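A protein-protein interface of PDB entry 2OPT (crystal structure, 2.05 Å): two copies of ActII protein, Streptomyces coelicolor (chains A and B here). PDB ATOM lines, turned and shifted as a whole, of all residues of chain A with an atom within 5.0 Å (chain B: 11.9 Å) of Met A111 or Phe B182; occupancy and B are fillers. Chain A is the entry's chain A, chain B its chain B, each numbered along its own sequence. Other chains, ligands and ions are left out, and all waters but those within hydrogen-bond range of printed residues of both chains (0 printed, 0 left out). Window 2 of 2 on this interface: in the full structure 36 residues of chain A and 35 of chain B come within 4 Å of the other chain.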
ATOM      1  N   ASP A  59       2.585 -28.705 -20.916  1.00  0.00           N
ATOM      2  CA  ASP A  59       3.015 -29.019 -19.560  1.00  0.00           C
ATOM      3  C   ASP A  59       2.189 -30.113 -18.918  1.00  0.00           C
ATOM      4  O   ASP A  59       2.703 -30.924 -18.130  1.00  0.00           O
ATOM      5  CB  ASP A  59       2.990 -27.794 -18.670  1.00  0.00           C
ATOM      6  CG  ASP A  59       3.832 -27.998 -17.443  1.00  0.00           C
ATOM      7  OD1 ASP A  59       5.071 -28.078 -17.599  1.00  0.00           O
ATOM      8  OD2 ASP A  59       3.238 -28.244 -16.356  1.00  0.00           O
ATOM      9  N   PRO A 105      10.197 -26.804 -21.834  1.00  0.00           N
ATOM     10  CA  PRO A 105       9.299 -27.358 -20.834  1.00  0.00           C
ATOM     11  C   PRO A 105       9.614 -26.769 -19.459  1.00  0.00           C
ATOM     12  O   PRO A 105      10.206 -27.431 -18.615  1.00  0.00           O
ATOM     13  CB  PRO A 105       9.555 -28.878 -20.906  1.00  0.00           C
ATOM     14  CG  PRO A 105      10.909 -29.052 -21.537  1.00  0.00           C
ATOM     15  CD  PRO A 105      11.274 -27.747 -22.240  1.00  0.00           C
ATOM     16  N   LEU A 106       9.220 -25.518 -19.256  1.00  0.00           N
ATOM     17  CA  LEU A 106       9.381 -24.857 -17.969  1.00  0.00           C
ATOM     18  C   LEU A 106       8.045 -24.368 -17.366  1.00  0.00           C
ATOM     19  O   LEU A 106       7.993 -23.313 -16.727  1.00  0.00           O
ATOM     20  CB  LEU A 106      10.374 -23.705 -18.083  1.00  0.00           C
ATOM     21  CG  LEU A 106      11.818 -23.893 -17.598  1.00  0.00           C
ATOM     22  CD1 LEU A 106      12.240 -25.334 -17.221  1.00  0.00           C
ATOM     23  CD2 LEU A 106      12.751 -23.336 -18.639  1.00  0.00           C
ATOM     24  N   GLY A 107       6.961 -25.104 -17.595  1.00  0.00           N
ATOM     25  CA  GLY A 107       5.838 -24.983 -16.701  1.00  0.00           C
ATOM     26  C   GLY A 107       6.116 -25.904 -15.503  1.00  0.00           C
ATOM     27  O   GLY A 107       7.179 -26.499 -15.402  1.00  0.00           O
ATOM     28  N   PRO A 108       5.126 -26.063 -14.619  1.00  0.00           N
ATOM     29  CA  PRO A 108       5.197 -26.858 -13.398  1.00  0.00           C
ATOM     30  C   PRO A 108       5.756 -28.228 -13.623  1.00  0.00           C
ATOM     31  O   PRO A 108       6.754 -28.579 -13.033  1.00  0.00           O
ATOM     32  CB  PRO A 108       3.743 -26.976 -12.974  1.00  0.00           C
ATOM     33  CG  PRO A 108       3.036 -25.798 -13.625  1.00  0.00           C
ATOM     34  CD  PRO A 108       3.809 -25.408 -14.809  1.00  0.00           C
ATOM     35  N   ASN A 109       5.111 -29.032 -14.460  1.00  0.00           N
ATOM     36  CA  ASN A 109       5.570 -30.402 -14.642  1.00  0.00           C
ATOM     37  C   ASN A 109       6.919 -30.424 -15.346  1.00  0.00           C
ATOM     38  O   ASN A 109       7.787 -31.264 -15.040  1.00  0.00           O
ATOM     39  CB  ASN A 109       4.554 -31.218 -15.413  1.00  0.00           C
ATOM     40  CG  ASN A 109       3.365 -31.496 -14.603  1.00  0.00           C
ATOM     41  OD1 ASN A 109       3.457 -31.853 -13.419  1.00  0.00           O
ATOM     42  ND2 ASN A 109       2.206 -31.282 -15.201  1.00  0.00           N
ATOM     43  N   GLY A 110       7.104 -29.459 -16.240  1.00  0.00           N
ATOM     44  CA  GLY A 110       8.337 -29.411 -16.998  1.00  0.00           C
ATOM     45  C   GLY A 110       9.529 -29.100 -16.118  1.00  0.00           C
ATOM     46  O   GLY A 110      10.586 -29.730 -16.280  1.00  0.00           O
ATOM     47  N   MET A 111       9.406 -28.051 -15.290  1.00  0.00           N
ATOM     48  CA  MET A 111      10.511 -27.654 -14.449  1.00  0.00           C
ATOM     49  C   MET A 111      10.885 -28.757 -13.437  1.00  0.00           C
ATOM     50  O   MET A 111      12.034 -29.018 -13.253  1.00  0.00           O
ATOM     51  CB  MET A 111      10.250 -26.285 -13.802  1.00  0.00           C
ATOM     52  CG  MET A 111       9.116 -26.261 -12.769  1.00  0.00           C
ATOM     53  SD  MET A 111       9.007 -24.752 -11.783  1.00  0.00           S
ATOM     54  CE  MET A 111      10.763 -24.425 -11.444  1.00  0.00           C
ATOM     55  N   VAL A 112       9.923 -29.423 -12.808  1.00  0.00           N
ATOM     56  CA  VAL A 112      10.227 -30.541 -11.916  1.00  0.00           C
ATOM     57  C   VAL A 112      10.954 -31.635 -12.715  1.00  0.00           C
ATOM     58  O   VAL A 112      11.967 -32.192 -12.273  1.00  0.00           O
ATOM     59  CB  VAL A 112       8.909 -31.108 -11.261  1.00  0.00           C
ATOM     60  CG1 VAL A 112       9.171 -32.398 -10.486  1.00  0.00           C
ATOM     61  CG2 VAL A 112       8.263 -30.034 -10.370  1.00  0.00           C
ATOM     62  N   GLY A 113      10.488 -31.897 -13.935  1.00  0.00           N
ATOM     63  CA  GLY A 113      11.063 -32.954 -14.762  1.00  0.00           C
ATOM     64  C   GLY A 113      12.507 -32.628 -15.087  1.00  0.00           C
ATOM     65  O   GLY A 113      13.347 -33.500 -15.117  1.00  0.00           O
ATOM     66  N   MET A 114      12.783 -31.364 -15.343  1.00  0.00           N
ATOM     67  CA  MET A 114      14.104 -30.936 -15.702  1.00  0.00           C
ATOM     68  C   MET A 114      15.038 -31.005 -14.484  1.00  0.00           C
ATOM     69  O   MET A 114      16.192 -31.428 -14.582  1.00  0.00           O
ATOM     70  CB  MET A 114      14.085 -29.516 -16.282  1.00  0.00           C
ATOM     71  CG  MET A 114      15.395 -29.255 -17.077  1.00  0.00           C
ATOM     72  SD  MET A 114      15.484 -27.644 -17.904  1.00  0.00           S
ATOM     73  CE  MET A 114      13.898 -27.580 -18.743  1.00  0.00           C
ATOM     74  N   GLU A 115      14.554 -30.570 -13.338  1.00  0.00           N
ATOM     75  CA  GLU A 115      15.321 -30.726 -12.107  1.00  0.00           C
ATOM     76  C   GLU A 115      15.733 -32.175 -11.867  1.00  0.00           C
ATOM     77  O   GLU A 115      16.862 -32.461 -11.535  1.00  0.00           O
ATOM     78  CB  GLU A 115      14.515 -30.170 -10.944  1.00  0.00           C
ATOM     79  CG  GLU A 115      15.194 -30.220  -9.546  1.00  0.00           C
ATOM     80  CD  GLU A 115      16.483 -29.481  -9.444  1.00  0.00           C
ATOM     81  OE1 GLU A 115      16.696 -28.458 -10.120  1.00  0.00           O
ATOM     82  OE2 GLU A 115      17.302 -29.914  -8.606  1.00  0.00           O
ATOM     83  N   GLN B 169      16.374 -13.909 -20.205  1.00  0.00           N
ATOM     84  CA  GLN B 169      15.269 -13.885 -19.221  1.00  0.00           C
ATOM     85  C   GLN B 169      15.055 -15.283 -18.643  1.00  0.00           C
ATOM     86  O   GLN B 169      14.653 -15.456 -17.494  1.00  0.00           O
ATOM     87  CB  GLN B 169      13.966 -13.367 -19.853  1.00  0.00           C
ATOM     88  CG  GLN B 169      14.093 -12.038 -20.614  1.00  0.00           C
ATOM     89  CD  GLN B 169      12.986 -11.057 -20.271  1.00  0.00           C
ATOM     90  OE1 GLN B 169      12.416 -11.104 -19.174  1.00  0.00           O
ATOM     91  NE2 GLN B 169      12.691 -10.140 -21.194  1.00  0.00           N
ATOM     92  N   LEU B 170      15.342 -16.272 -19.477  1.00  0.00           N
ATOM     93  CA  LEU B 170      15.357 -17.653 -19.096  1.00  0.00           C
ATOM     94  C   LEU B 170      16.424 -17.920 -18.009  1.00  0.00           C
ATOM     95  O   LEU B 170      16.161 -18.623 -17.032  1.00  0.00           O
ATOM     96  CB  LEU B 170      15.580 -18.491 -20.352  1.00  0.00           C
ATOM     97  CG  LEU B 170      14.833 -19.816 -20.435  1.00  0.00           C
ATOM     98  CD1 LEU B 170      15.770 -21.008 -20.269  1.00  0.00           C
ATOM     99  CD2 LEU B 170      13.669 -19.880 -19.445  1.00  0.00           C
ATOM    100  N   HIS B 171      17.597 -17.332 -18.178  1.00  0.00           N
ATOM    101  CA  HIS B 171      18.674 -17.335 -17.190  1.00  0.00           C
ATOM    102  C   HIS B 171      18.236 -16.775 -15.838  1.00  0.00           C
ATOM    103  O   HIS B 171      18.323 -17.484 -14.842  1.00  0.00           O
ATOM    104  CB  HIS B 171      19.896 -16.561 -17.728  1.00  0.00           C
ATOM    105  CG  HIS B 171      21.190 -16.852 -17.020  1.00  0.00           C
ATOM    106  ND1 HIS B 171      21.288 -17.009 -15.655  1.00  0.00           N
ATOM    107  CD2 HIS B 171      22.455 -16.957 -17.495  1.00  0.00           C
ATOM    108  CE1 HIS B 171      22.545 -17.237 -15.322  1.00  0.00           C
ATOM    109  NE2 HIS B 171      23.276 -17.199 -16.419  1.00  0.00           N
ATOM    110  N   GLY B 172      17.785 -15.520 -15.795  1.00  0.00           N
ATOM    111  CA  GLY B 172      17.351 -14.909 -14.530  1.00  0.00           C
ATOM    112  C   GLY B 172      16.291 -15.715 -13.799  1.00  0.00           C
ATOM    113  O   GLY B 172      16.354 -15.894 -12.578  1.00  0.00           O
ATOM    114  N   TYR B 173      15.325 -16.219 -14.566  1.00  0.00           N
ATOM    115  CA  TYR B 173      14.263 -17.050 -14.027  1.00  0.00           C
ATOM    116  C   TYR B 173      14.827 -18.255 -13.261  1.00  0.00           C
ATOM    117  O   TYR B 173      14.474 -18.500 -12.091  1.00  0.00           O
ATOM    118  CB  TYR B 173      13.361 -17.555 -15.159  1.00  0.00           C
ATOM    119  CG  TYR B 173      12.270 -18.450 -14.637  1.00  0.00           C
ATOM    120  CD1 TYR B 173      11.209 -17.917 -13.923  1.00  0.00           C
ATOM    121  CD2 TYR B 173      12.315 -19.813 -14.825  1.00  0.00           C
ATOM    122  CE1 TYR B 173      10.227 -18.694 -13.434  1.00  0.00           C
ATOM    123  CE2 TYR B 173      11.317 -20.633 -14.333  1.00  0.00           C
ATOM    124  CZ  TYR B 173      10.277 -20.054 -13.633  1.00  0.00           C
ATOM    125  OH  TYR B 173       9.262 -20.797 -13.125  1.00  0.00           O
ATOM    126  N   LEU B 174      15.685 -19.015 -13.941  1.00  0.00           N
ATOM    127  CA  LEU B 174      16.270 -20.245 -13.380  1.00  0.00           C
ATOM    128  C   LEU B 174      17.168 -19.936 -12.187  1.00  0.00           C
ATOM    129  O   LEU B 174      17.137 -20.641 -11.194  1.00  0.00           O
ATOM    130  CB  LEU B 174      17.053 -21.015 -14.454  1.00  0.00           C
ATOM    131  CG  LEU B 174      16.270 -21.648 -15.605  1.00  0.00           C
ATOM    132  CD1 LEU B 174      17.210 -22.306 -16.641  1.00  0.00           C
ATOM    133  CD2 LEU B 174      15.197 -22.637 -15.066  1.00  0.00           C
ATOM    134  N   LYS B 175      17.971 -18.874 -12.298  1.00  0.00           N
ATOM    135  CA  LYS B 175      18.894 -18.510 -11.231  1.00  0.00           C
ATOM    136  C   LYS B 175      18.168 -18.134  -9.940  1.00  0.00           C
ATOM    137  O   LYS B 175      18.724 -18.305  -8.839  1.00  0.00           O
ATOM    138  CB  LYS B 175      19.860 -17.365 -11.669  1.00  0.00           C
ATOM    139  N   SER B 176      16.937 -17.633 -10.048  1.00  0.00           N
ATOM    140  CA  SER B 176      16.239 -17.148  -8.868  1.00  0.00           C
ATOM    141  C   SER B 176      15.206 -18.130  -8.310  1.00  0.00           C
ATOM    142  O   SER B 176      14.382 -17.770  -7.475  1.00  0.00           O
ATOM    143  CB  SER B 176      15.593 -15.821  -9.183  1.00  0.00           C
ATOM    144  OG  SER B 176      14.465 -16.089  -9.979  1.00  0.00           O
ATOM    145  N   LEU B 177      15.244 -19.370  -8.785  1.00  0.00           N
ATOM    146  CA  LEU B 177      14.438 -20.435  -8.249  1.00  0.00           C
ATOM    147  C   LEU B 177      14.890 -20.751  -6.821  1.00  0.00           C
ATOM    148  O   LEU B 177      16.085 -20.598  -6.509  1.00  0.00           O
ATOM    149  CB  LEU B 177      14.602 -21.656  -9.152  1.00  0.00           C
ATOM    150  CG  LEU B 177      13.481 -22.137 -10.097  1.00  0.00           C
ATOM    151  CD1 LEU B 177      12.400 -21.135 -10.484  1.00  0.00           C
ATOM    152  CD2 LEU B 177      14.080 -22.878 -11.326  1.00  0.00           C
ATOM    153  N   PRO B 178      13.959 -21.187  -5.943  1.00  0.00           N
ATOM    154  CA  PRO B 178      14.397 -21.569  -4.594  1.00  0.00           C
ATOM    155  C   PRO B 178      15.435 -22.719  -4.641  1.00  0.00           C
ATOM    156  O   PRO B 178      15.103 -23.874  -4.966  1.00  0.00           O
ATOM    157  CB  PRO B 178      13.074 -21.984  -3.881  1.00  0.00           C
ATOM    158  CG  PRO B 178      12.131 -22.268  -4.964  1.00  0.00           C
ATOM    159  CD  PRO B 178      12.513 -21.399  -6.131  1.00  0.00           C
ATOM    160  N   ALA B 179      16.682 -22.387  -4.316  1.00  0.00           N
ATOM    161  CA  ALA B 179      17.829 -23.290  -4.456  1.00  0.00           C
ATOM    162  C   ALA B 179      17.689 -24.606  -3.694  1.00  0.00           C
ATOM    163  O   ALA B 179      18.295 -25.620  -4.054  1.00  0.00           O
ATOM    164  CB  ALA B 179      19.061 -22.580  -4.018  1.00  0.00           C
ATOM    165  N   THR B 180      16.866 -24.594  -2.651  1.00  0.00           N
ATOM    166  CA  THR B 180      16.603 -25.782  -1.856  1.00  0.00           C
ATOM    167  C   THR B 180      15.648 -26.732  -2.595  1.00  0.00           C
ATOM    168  O   THR B 180      15.681 -27.971  -2.424  1.00  0.00           O
ATOM    169  CB  THR B 180      15.992 -25.363  -0.487  1.00  0.00           C
ATOM    170  OG1 THR B 180      16.988 -24.687   0.303  1.00  0.00           O
ATOM    171  CG2 THR B 180      15.533 -26.552   0.272  1.00  0.00           C
ATOM    172  N   SER B 181      14.770 -26.168  -3.413  1.00  0.00           N
ATOM    173  CA  SER B 181      13.866 -27.009  -4.173  1.00  0.00           C
ATOM    174  C   SER B 181      14.391 -27.331  -5.577  1.00  0.00           C
ATOM    175  O   SER B 181      14.094 -28.392  -6.132  1.00  0.00           O
ATOM    176  CB  SER B 181      12.452 -26.404  -4.221  1.00  0.00           C
ATOM    177  OG  SER B 181      11.894 -26.356  -2.900  1.00  0.00           O
ATOM    178  N   PHE B 182      15.150 -26.422  -6.164  1.00  0.00           N
ATOM    179  CA  PHE B 182      15.691 -26.647  -7.515  1.00  0.00           C
ATOM    180  C   PHE B 182      17.205 -26.413  -7.564  1.00  0.00           C
ATOM    181  O   PHE B 182      17.658 -25.503  -8.293  1.00  0.00           O
ATOM    182  CB  PHE B 182      14.937 -25.750  -8.524  1.00  0.00           C
ATOM    183  CG  PHE B 182      13.451 -25.939  -8.457  1.00  0.00           C
ATOM    184  CD1 PHE B 182      12.684 -25.215  -7.549  1.00  0.00           C
ATOM    185  CD2 PHE B 182      12.819 -26.882  -9.265  1.00  0.00           C
ATOM    186  CE1 PHE B 182      11.305 -25.418  -7.467  1.00  0.00           C
ATOM    187  CE2 PHE B 182      11.447 -27.117  -9.173  1.00  0.00           C
ATOM    188  CZ  PHE B 182      10.696 -26.399  -8.241  1.00  0.00           C
ATOM    189  N   PRO B 183      17.997 -27.192  -6.767  1.00  0.00           N
ATOM    190  CA  PRO B 183      19.450 -26.886  -6.684  1.00  0.00           C
ATOM    191  C   PRO B 183      20.152 -27.106  -8.035  1.00  0.00           C
ATOM    192  O   PRO B 183      21.047 -26.362  -8.416  1.00  0.00           O
ATOM    193  CB  PRO B 183      19.929 -27.851  -5.607  1.00  0.00           C
ATOM    194  CG  PRO B 183      18.931 -28.959  -5.640  1.00  0.00           C
ATOM    195  CD  PRO B 183      17.641 -28.287  -5.857  1.00  0.00           C
ATOM    196  N   ASN B 184      19.730 -28.117  -8.790  1.00  0.00           N
ATOM    197  CA  ASN B 184      20.379 -28.365 -10.080  1.00  0.00           C
ATOM    198  C   ASN B 184      20.044 -27.307 -11.108  1.00  0.00           C
ATOM    199  O   ASN B 184      20.927 -26.899 -11.869  1.00  0.00           O
ATOM    200  CB  ASN B 184      20.037 -29.771 -10.620  1.00  0.00           C
ATOM    201  CG  ASN B 184      20.647 -30.845  -9.782  1.00  0.00           C
ATOM    202  OD1 ASN B 184      21.824 -31.164  -9.926  1.00  0.00           O
ATOM    203  ND2 ASN B 184      19.858 -31.410  -8.886  1.00  0.00           N
ATOM    204  N   LEU B 185      18.768 -26.894 -11.200  1.00  0.00           N
ATOM    205  CA  LEU B 185      18.419 -25.823 -12.166  1.00  0.00           C
ATOM    206  C   LEU B 185      19.068 -24.507 -11.808  1.00  0.00           C
ATOM    207  O   LEU B 185      19.502 -23.739 -12.674  1.00  0.00           O
ATOM    208  CB  LEU B 185      16.917 -25.625 -12.259  1.00  0.00           C
ATOM    209  CG  LEU B 185      16.146 -26.474 -13.260  1.00  0.00           C
ATOM    210  CD1 LEU B 185      16.930 -27.600 -13.848  1.00  0.00           C
ATOM    211  CD2 LEU B 185      14.967 -26.919 -12.587  1.00  0.00           C
ATOM    212  N   VAL B 186      19.170 -24.216 -10.527  1.00  0.00           N
ATOM    213  CA  VAL B 186      19.884 -22.974 -10.150  1.00  0.00           C
ATOM    214  C   VAL B 186      21.345 -23.064 -10.545  1.00  0.00           C
ATOM    215  O   VAL B 186      21.899 -22.168 -11.211  1.00  0.00           O
ATOM    216  CB  VAL B 186      19.747 -22.685  -8.640  1.00  0.00           C
ATOM    217  CG1 VAL B 186      20.557 -21.479  -8.230  1.00  0.00           C
ATOM    218  CG2 VAL B 186      18.270 -22.526  -8.256  1.00  0.00           C
ATOM    219  N   HIS B 187      21.997 -24.130 -10.113  1.00  0.00           N
ATOM    220  CA  HIS B 187      23.419 -24.318 -10.399  1.00  0.00           C
ATOM    221  C   HIS B 187      23.772 -24.313 -11.906  1.00  0.00           C
ATOM    222  O   HIS B 187      24.755 -23.680 -12.323  1.00  0.00           O
ATOM    223  CB  HIS B 187      23.907 -25.607  -9.727  1.00  0.00           C
ATOM    224  CG  HIS B 187      25.359 -25.880  -9.956  1.00  0.00           C
ATOM    225  ND1 HIS B 187      26.352 -25.232  -9.257  1.00  0.00           N
ATOM    226  CD2 HIS B 187      25.984 -26.694 -10.838  1.00  0.00           C
ATOM    227  CE1 HIS B 187      27.531 -25.656  -9.680  1.00  0.00           C
ATOM    228  NE2 HIS B 187      27.335 -26.543 -10.641  1.00  0.00           N
ATOM    229  N   LEU B 188      22.954 -25.006 -12.711  1.00  0.00           N
ATOM    230  CA  LEU B 188      23.177 -25.120 -14.155  1.00  0.00           C
ATOM    231  C   LEU B 188      22.498 -24.003 -14.961  1.00  0.00           C
ATOM    232  O   LEU B 188      22.292 -24.150 -16.170  1.00  0.00           O
ATOM    233  CB  LEU B 188      22.686 -26.506 -14.641  1.00  0.00           C
ATOM    234  CG  LEU B 188      23.423 -27.702 -14.025  1.00  0.00           C
ATOM    235  CD1 LEU B 188      22.813 -29.058 -14.402  1.00  0.00           C
ATOM    236  CD2 LEU B 188      24.890 -27.603 -14.482  1.00  0.00           C
ATOM    237  N   ALA B 189      22.059 -22.943 -14.281  1.00  0.00           N
ATOM    238  CA  ALA B 189      21.227 -21.914 -14.912  1.00  0.00           C
ATOM    239  C   ALA B 189      21.860 -21.395 -16.228  1.00  0.00           C
ATOM    240  O   ALA B 189      21.186 -21.299 -17.275  1.00  0.00           O
ATOM    241  CB  ALA B 189      21.025 -20.734 -13.947  1.00  0.00           C
ATOM    242  N   GLY B 190      23.149 -21.069 -16.141  1.00  0.00           N
ATOM    243  CA  GLY B 190      23.953 -20.574 -17.285  1.00  0.00           C
ATOM    244  C   GLY B 190      24.048 -21.566 -18.452  1.00  0.00           C
ATOM    245  O   GLY B 190      23.574 -21.269 -19.537  1.00  0.00           O
ATOM    246  N   ILE B 192      22.332 -24.222 -19.180  1.00  0.00           N
ATOM    247  CA  ILE B 192      21.018 -24.610 -19.710  1.00  0.00           C
ATOM    248  C   ILE B 192      20.508 -23.563 -20.705  1.00  0.00           C
ATOM    249  O   ILE B 192      20.039 -23.893 -21.806  1.00  0.00           O
ATOM    250  CB  ILE B 192      20.004 -24.856 -18.567  1.00  0.00           C
ATOM    251  CG1 ILE B 192      20.357 -26.152 -17.810  1.00  0.00           C
ATOM    252  CG2 ILE B 192      18.568 -24.908 -19.099  1.00  0.00           C
ATOM    253  CD1 ILE B 192      19.575 -26.381 -16.563  1.00  0.00           C
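Among the printed residues, merely in contact across the chains: Leu A106 with Leu B170, Met A111 with Leu B177, Met A111 with Phe B182, Met A111 with Leu B185, Met A114 with Leu B185 and Glu A115 with Phe B182.
Of the 23 printed residues of chain B, 6 touch a printed residue of chain A.
Hydrophobic or aromatic side chains of chain B that line the printed part of chain A: Leu B170, Leu B177, Phe B182, Pro B183 and Leu B185.
Along chain B the printed residues that touch a printed residue of chain A span positions 170 to 185.
Printed residues of chain A that touch a printed residue of chain B: Leu A106, Met A111, Met A114 and Glu A115.
Hydrophobic or aromatic side chains of chain A within 4 Å of the printed part of chain B: Leu A106, Met A111 and Met A114.
Among the printed residues, no Asp or Glu carboxylate lies within 4 Å of a Lys or Arg side-chain nitrogen of the other chain.
Printed residues of chain B within 4 Å of Met A111: Leu B177 (3.7 Å), Phe B182 (3.6 Å) and Leu B185 (3.7 Å).
Printed residues of chain A within 4 Å of Phe B182: Met A111 (3.6 Å) and Glu A115 (3.3 Å).
Pro A105 touches none of the printed residues of chain B.
No residue of chain B comes within 4 Å of Pro A108.
No residue of chain B comes within 4 Å of Gly A110.
No residue of chain B comes within 4 Å of Gly A113.
Met A114 touches just one residue of chain B: Leu B185.
Of chain B, only Phe B182 (3.3 Å), Pro B183 (3.2 Å), Asn B184 (3.0 Å) and Leu B185 (2.8 Å) come within 4 Å of Glu A115.
Printed residues of chain A within 4 Å of Asn B184: Glu A115.
Printed residues of chain A within 4 Å of Leu B185: Met A111 (3.7 Å), Met A114 (3.9 Å) and Glu A115 (2.8 Å).
Printed residues of chain A within 4 Å of Leu B177: Met A111.
Gly B190 touches none of the printed residues of chain A.
Val B186 touches none of the printed residues of chain A.
The nearest printed residue of chain A that does not touch Phe B182 is Val A112 (4.5 Å).
The nearest printed residue of chain A that does not touch Leu B177 is Glu A115 (6.3 Å).
No position is printed for both chains.
N of Met A111 lies within hydrogen-bond range of O of Pro A105 (3.5 Å).
N of Leu B185 lies within hydrogen-bond range of OE1 of Glu A115, 2.8 Å away.
The backbone nitrogen of Pro B183 sits close to the side-chain carboxylate of Glu A115 (3.4 Å).
The side-chain carboxylate of Glu A115 lies within hydrogen-bond range of the side-chain amide nitrogen of Asn B184 (3.0 Å).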
